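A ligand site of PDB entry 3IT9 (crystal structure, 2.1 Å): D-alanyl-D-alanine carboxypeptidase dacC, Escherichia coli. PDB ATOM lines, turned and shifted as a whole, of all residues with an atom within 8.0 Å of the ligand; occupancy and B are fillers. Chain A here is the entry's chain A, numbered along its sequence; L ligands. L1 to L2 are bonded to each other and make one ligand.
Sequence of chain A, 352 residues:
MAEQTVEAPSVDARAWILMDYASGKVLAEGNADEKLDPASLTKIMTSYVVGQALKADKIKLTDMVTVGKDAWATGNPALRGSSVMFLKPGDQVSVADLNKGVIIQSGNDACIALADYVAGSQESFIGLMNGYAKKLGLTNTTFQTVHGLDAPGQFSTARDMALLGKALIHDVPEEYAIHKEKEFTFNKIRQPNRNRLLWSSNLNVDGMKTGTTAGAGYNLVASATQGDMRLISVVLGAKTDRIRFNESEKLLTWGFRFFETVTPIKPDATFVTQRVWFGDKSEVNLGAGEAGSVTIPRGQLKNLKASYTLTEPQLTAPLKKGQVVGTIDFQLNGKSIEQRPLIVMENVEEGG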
ATOM      1  N   ASN A 195      13.292  -9.657  -2.442  1.00  0.00           N
ATOM      2  CA  ASN A 195      14.651  -9.415  -1.886  1.00  0.00           C
ATOM      3  C   ASN A 195      14.935  -7.956  -1.578  1.00  0.00           C
ATOM      4  O   ASN A 195      15.471  -7.241  -2.400  1.00  0.00           O
ATOM      5  CB  ASN A 195      15.731  -9.971  -2.829  1.00  0.00           C
ATOM      6  CG  ASN A 195      17.130  -9.909  -2.229  1.00  0.00           C
ATOM      7  OD1 ASN A 195      17.299  -9.554  -1.040  1.00  0.00           O
ATOM      8  ND2 ASN A 195      18.132 -10.255  -3.026  1.00  0.00           N
ATOM      9  N   ARG A 196      14.630  -7.544  -0.356  1.00  0.00           N
ATOM     10  CA  ARG A 196      14.711  -6.134   0.038  1.00  0.00           C
ATOM     11  C   ARG A 196      16.142  -5.626  -0.012  1.00  0.00           C
ATOM     12  O   ARG A 196      16.378  -4.417  -0.085  1.00  0.00           O
ATOM     13  CB  ARG A 196      14.129  -5.948   1.436  1.00  0.00           C
ATOM     14  CG  ARG A 196      12.661  -6.410   1.568  1.00  0.00           C
ATOM     15  CD  ARG A 196      11.714  -5.497   0.794  1.00  0.00           C
ATOM     16  NE  ARG A 196      11.950  -4.095   1.133  1.00  0.00           N
ATOM     17  CZ  ARG A 196      11.739  -3.070   0.308  1.00  0.00           C
ATOM     18  NH1 ARG A 196      11.258  -3.287  -0.929  1.00  0.00           N
ATOM     19  NH2 ARG A 196      11.974  -1.818   0.727  1.00  0.00           N
ATOM     20  N   LEU A 197      17.099  -6.542   0.022  1.00  0.00           N
ATOM     21  CA  LEU A 197      18.511  -6.173   0.034  1.00  0.00           C
ATOM     22  C   LEU A 197      18.946  -5.565  -1.298  1.00  0.00           C
ATOM     23  O   LEU A 197      19.974  -4.868  -1.363  1.00  0.00           O
ATOM     24  CB  LEU A 197      19.364  -7.391   0.395  1.00  0.00           C
ATOM     25  CG  LEU A 197      20.328  -7.182   1.556  1.00  0.00           C
ATOM     26  CD1 LEU A 197      19.645  -6.434   2.667  1.00  0.00           C
ATOM     27  CD2 LEU A 197      20.890  -8.516   2.055  1.00  0.00           C
ATOM     28  N   LEU A 198      18.163  -5.803  -2.349  1.00  0.00           N
ATOM     29  CA  LEU A 198      18.401  -5.117  -3.640  1.00  0.00           C
ATOM     30  C   LEU A 198      18.319  -3.593  -3.511  1.00  0.00           C
ATOM     31  O   LEU A 198      18.844  -2.846  -4.357  1.00  0.00           O
ATOM     32  CB  LEU A 198      17.415  -5.604  -4.714  1.00  0.00           C
ATOM     33  CG  LEU A 198      17.494  -7.098  -5.107  1.00  0.00           C
ATOM     34  CD1 LEU A 198      16.350  -7.448  -6.046  1.00  0.00           C
ATOM     35  CD2 LEU A 198      18.854  -7.435  -5.758  1.00  0.00           C
ATOM     36  N   TRP A 199      17.646  -3.131  -2.465  1.00  0.00           N
ATOM     37  CA  TRP A 199      17.459  -1.676  -2.259  1.00  0.00           C
ATOM     38  C   TRP A 199      18.461  -1.105  -1.276  1.00  0.00           C
ATOM     39  O   TRP A 199      18.361   0.048  -0.900  1.00  0.00           O
ATOM     40  CB  TRP A 199      16.030  -1.372  -1.754  1.00  0.00           C
ATOM     41  CG  TRP A 199      14.979  -1.433  -2.828  1.00  0.00           C
ATOM     42  CD1 TRP A 199      14.528  -0.396  -3.591  1.00  0.00           C
ATOM     43  CD2 TRP A 199      14.267  -2.602  -3.269  1.00  0.00           C
ATOM     44  NE1 TRP A 199      13.569  -0.836  -4.482  1.00  0.00           N
ATOM     45  CE2 TRP A 199      13.389  -2.185  -4.302  1.00  0.00           C
ATOM     46  CE3 TRP A 199      14.269  -3.940  -2.882  1.00  0.00           C
ATOM     47  CZ2 TRP A 199      12.535  -3.074  -4.959  1.00  0.00           C
ATOM     48  CZ3 TRP A 199      13.431  -4.828  -3.532  1.00  0.00           C
ATOM     49  CH2 TRP A 199      12.567  -4.385  -4.573  1.00  0.00           C
ATOM     50  N   SER A 200      19.389  -1.935  -0.825  1.00  0.00           N
ATOM     51  CA  SER A 200      20.404  -1.487   0.157  1.00  0.00           C
ATOM     52  C   SER A 200      21.284  -0.427  -0.420  1.00  0.00           C
ATOM     53  O   SER A 200      21.826  -0.589  -1.501  1.00  0.00           O
ATOM     54  CB  SER A 200      21.265  -2.660   0.643  1.00  0.00           C
ATOM     55  OG  SER A 200      20.466  -3.608   1.327  1.00  0.00           O
ATOM     56  N   SER A 201      21.467   0.649   0.323  1.00  0.00           N
ATOM     57  CA  SER A 201      22.371   1.713  -0.072  1.00  0.00           C
ATOM     58  C   SER A 201      23.818   1.431   0.351  1.00  0.00           C
ATOM     59  O   SER A 201      24.764   1.959  -0.249  1.00  0.00           O
ATOM     60  CB  SER A 201      21.907   3.045   0.541  1.00  0.00           C
ATOM     61  OG  SER A 201      21.055   3.737  -0.360  1.00  0.00           O
ATOM     62  N   ASN A 202      23.996   0.628   1.392  1.00  0.00           N
ATOM     63  CA  ASN A 202      25.337   0.355   1.963  1.00  0.00           C
ATOM     64  C   ASN A 202      26.039  -0.884   1.383  1.00  0.00           C
ATOM     65  O   ASN A 202      27.123  -1.251   1.830  1.00  0.00           O
ATOM     66  CB  ASN A 202      25.259   0.253   3.476  1.00  0.00           C
ATOM     67  CG  ASN A 202      24.612   1.473   4.119  1.00  0.00           C
ATOM     68  OD1 ASN A 202      24.747   2.600   3.626  1.00  0.00           O
ATOM     69  ND2 ASN A 202      23.872   1.254   5.210  1.00  0.00           N
ATOM     70  N   LEU A 203      25.396  -1.522   0.405  1.00  0.00           N
ATOM     71  CA  LEU A 203      25.973  -2.655  -0.322  1.00  0.00           C
ATOM     72  C   LEU A 203      25.495  -2.610  -1.773  1.00  0.00           C
ATOM     73  O   LEU A 203      24.366  -2.180  -2.045  1.00  0.00           O
ATOM     74  CB  LEU A 203      25.497  -3.958   0.291  1.00  0.00           C
ATOM     75  CG  LEU A 203      26.025  -4.333   1.676  1.00  0.00           C
ATOM     76  CD1 LEU A 203      25.340  -5.619   2.156  1.00  0.00           C
ATOM     77  CD2 LEU A 203      27.550  -4.495   1.644  1.00  0.00           C
ATOM     78  N   VAL A 205      24.136  -5.135  -3.718  1.00  0.00           N
ATOM     79  CA  VAL A 205      23.556  -6.478  -3.720  1.00  0.00           C
ATOM     80  C   VAL A 205      22.864  -6.749  -5.045  1.00  0.00           C
ATOM     81  O   VAL A 205      22.149  -5.887  -5.561  1.00  0.00           O
ATOM     82  CB  VAL A 205      22.533  -6.575  -2.598  1.00  0.00           C
ATOM     83  CG1 VAL A 205      21.839  -7.884  -2.633  1.00  0.00           C
ATOM     84  CG2 VAL A 205      23.210  -6.331  -1.264  1.00  0.00           C
ATOM     85  N   ASP A 241      11.648 -11.447   9.470  1.00  0.00           N
ATOM     86  CA  ASP A 241      12.014 -10.888   8.173  1.00  0.00           C
ATOM     87  C   ASP A 241      13.108  -9.826   8.298  1.00  0.00           C
ATOM     88  O   ASP A 241      14.110  -9.864   7.569  1.00  0.00           O
ATOM     89  CB  ASP A 241      10.748 -10.290   7.507  1.00  0.00           C
ATOM     90  CG  ASP A 241      11.011  -9.796   6.120  1.00  0.00           C
ATOM     91  OD1 ASP A 241      11.271 -10.632   5.234  1.00  0.00           O
ATOM     92  OD2 ASP A 241      10.974  -8.573   5.918  1.00  0.00           O
ATOM     93  N   ARG A 242      12.936  -8.912   9.233  1.00  0.00           N
ATOM     94  CA  ARG A 242      13.939  -7.894   9.490  1.00  0.00           C
ATOM     95  C   ARG A 242      15.316  -8.465   9.855  1.00  0.00           C
ATOM     96  O   ARG A 242      16.347  -7.946   9.416  1.00  0.00           O
ATOM     97  CB  ARG A 242      13.460  -6.921  10.566  1.00  0.00           C
ATOM     98  CG  ARG A 242      14.530  -5.928  11.010  1.00  0.00           C
ATOM     99  CD  ARG A 242      14.015  -5.016  12.106  1.00  0.00           C
ATOM    100  NE  ARG A 242      13.493  -3.765  11.550  1.00  0.00           N
ATOM    101  CZ  ARG A 242      14.244  -2.823  10.982  1.00  0.00           C
ATOM    102  NH1 ARG A 242      13.681  -1.731  10.495  1.00  0.00           N
ATOM    103  NH2 ARG A 242      15.563  -2.979  10.901  1.00  0.00           N
ATOM    104  N   PHE A 245      17.270  -9.994   6.935  1.00  0.00           N
ATOM    105  CA  PHE A 245      17.996  -9.054   6.081  1.00  0.00           C
ATOM    106  C   PHE A 245      19.200  -8.362   6.747  1.00  0.00           C
ATOM    107  O   PHE A 245      20.226  -8.152   6.115  1.00  0.00           O
ATOM    108  CB  PHE A 245      17.058  -8.001   5.477  1.00  0.00           C
ATOM    109  CG  PHE A 245      16.122  -8.552   4.455  1.00  0.00           C
ATOM    110  CD1 PHE A 245      16.610  -9.029   3.224  1.00  0.00           C
ATOM    111  CD2 PHE A 245      14.756  -8.615   4.701  1.00  0.00           C
ATOM    112  CE1 PHE A 245      15.746  -9.542   2.262  1.00  0.00           C
ATOM    113  CE2 PHE A 245      13.879  -9.142   3.744  1.00  0.00           C
ATOM    114  CZ  PHE A 245      14.369  -9.616   2.523  1.00  0.00           C
ATOM    115  N   ASN A 246      19.053  -7.915   7.990  1.00  0.00           N
ATOM    116  CA  ASN A 246      20.157  -7.191   8.579  1.00  0.00           C
ATOM    117  C   ASN A 246      21.357  -8.031   8.982  1.00  0.00           C
ATOM    118  O   ASN A 246      22.484  -7.580   8.886  1.00  0.00           O
ATOM    119  CB  ASN A 246      19.720  -6.209   9.676  1.00  0.00           C
ATOM    120  CG  ASN A 246      18.840  -6.847  10.697  1.00  0.00           C
ATOM    121  OD1 ASN A 246      17.659  -6.460  10.840  1.00  0.00           O
ATOM    122  ND2 ASN A 246      19.392  -7.793  11.462  1.00  0.00           N
ATOM    123  N   GLU A 249      23.010  -8.504   5.729  1.00  0.00           N
ATOM    124  CA  GLU A 249      23.687  -7.257   5.467  1.00  0.00           C
ATOM    125  C   GLU A 249      24.976  -7.164   6.253  1.00  0.00           C
ATOM    126  O   GLU A 249      26.007  -6.763   5.720  1.00  0.00           O
ATOM    127  CB  GLU A 249      22.783  -6.088   5.833  1.00  0.00           C
ATOM    128  CG  GLU A 249      22.648  -5.056   4.751  1.00  0.00           C
ATOM    129  CD  GLU A 249      23.278  -3.745   5.132  1.00  0.00           C
ATOM    130  OE1 GLU A 249      23.050  -2.750   4.411  1.00  0.00           O
ATOM    131  OE2 GLU A 249      24.003  -3.706   6.149  1.00  0.00           O
ATOM    132  N   THR A 253      28.879  -7.001   4.888  1.00  0.00           N
ATOM    133  CA  THR A 253      29.592  -5.759   5.139  1.00  0.00           C
ATOM    134  C   THR A 253      30.909  -6.070   5.846  1.00  0.00           C
ATOM    135  O   THR A 253      31.924  -5.500   5.525  1.00  0.00           O
ATOM    136  CB  THR A 253      28.735  -4.787   5.999  1.00  0.00           C
ATOM    137  OG1 THR A 253      27.799  -4.104   5.149  1.00  0.00           O
ATOM    138  CG2 THR A 253      29.610  -3.760   6.709  1.00  0.00           C
HETATM  139  C1  LIG L   1      17.177  -0.103   2.245  1.00  0.00           C
HETATM  140  C2  LIG L   1      15.674  -0.130   1.932  1.00  0.00           C
HETATM  141  C3  LIG L   1      14.927  -0.787   3.103  1.00  0.00           C
HETATM  142  C4  LIG L   1      15.495  -2.178   3.341  1.00  0.00           C
HETATM  143  C5  LIG L   1      17.005  -2.102   3.571  1.00  0.00           C
HETATM  144  C6  LIG L   1      17.577  -3.501   3.726  1.00  0.00           C
HETATM  145  O1  LIG L   1      15.189   1.201   1.697  1.00  0.00           O
HETATM  146  O2  LIG L   1      13.534  -0.890   2.821  1.00  0.00           O
HETATM  147  O3  LIG L   1      14.872  -2.790   4.466  1.00  0.00           O
HETATM  148  O4  LIG L   1      17.641  -1.452   2.457  1.00  0.00           O
HETATM  149  O5  LIG L   1      18.985  -3.441   3.513  1.00  0.00           O
HETATM  150  C1  LG2 L   2      17.981   2.704   2.265  1.00  0.00           C
HETATM  151  C2  LG2 L   2      18.389   1.677   3.337  1.00  0.00           C
HETATM  152  C3  LG2 L   2      18.567   2.331   4.709  1.00  0.00           C
HETATM  153  C4  LG2 L   2      19.599   1.456   5.395  1.00  0.00           C
HETATM  154  C5  LG2 L   2      20.360   0.766   4.256  1.00  0.00           C
HETATM  155  C6  LG2 L   2      20.395  -0.741   4.478  1.00  0.00           C
HETATM  156  O1  LG2 L   2      19.107   3.524   1.906  1.00  0.00           O
HETATM  157  O2  LG2 L   2      17.377   0.656   3.447  1.00  0.00           O
HETATM  158  O3  LG2 L   2      17.329   2.319   5.437  1.00  0.00           O
HETATM  159  O4  LG2 L   2      20.500   2.236   6.207  1.00  0.00           O
HETATM  160  O5  LG2 L   2      19.650   1.055   3.031  1.00  0.00           O
HETATM  161  O6  LG2 L   2      21.281  -1.322   3.520  1.00  0.00           O
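The side-chain carboxylate (OE1) of Glu 249 sits at hydrogen-bond distance from an oxygen (O6) of LG2 L2, at 2.4 Å. The guanidinium group of Arg 196 sits at hydrogen-bond distance from an oxygen (O2) of LIG L1 (2.8 Å). O5 of LG2 L2 is in hydrogen-bond range of N of Ser 201, at 3.3 Å. An oxygen (O5) of LIG L1 sits at hydrogen-bond distance from the side-chain hydroxyl of Ser 200, at 2.6 Å. OG of Ser 201 is in hydrogen-bond range of O1 of LG2 L2.
O of Glu 249 lies within hydrogen-bond range of OG1 of Thr 253. O of Leu 197 sits at hydrogen-bond distance from OG of Ser 200. The backbone NH of Leu 197 sits close to the side-chain amide oxygen of Asn 195, 3.2 Å away.
CD1 of Leu 197 touches O5 of LIG L1, at 3.2 Å. O of Trp 199 touches C1 of LIG L1 (3.4 Å). ND2 of Asn 202 touches O4 of LG2 L2, 3.7 Å away. Hydrophobic or aromatic side chains that line the ligand: Leu 197 and Trp 199. Within 4 Å of the ligand: Arg 196, Leu 197, Trp 199, Ser 200, Ser 201, Asn 202 and Glu 249. The nearest printed residue that does not touch the ligand is Phe 245 (4.9 Å).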
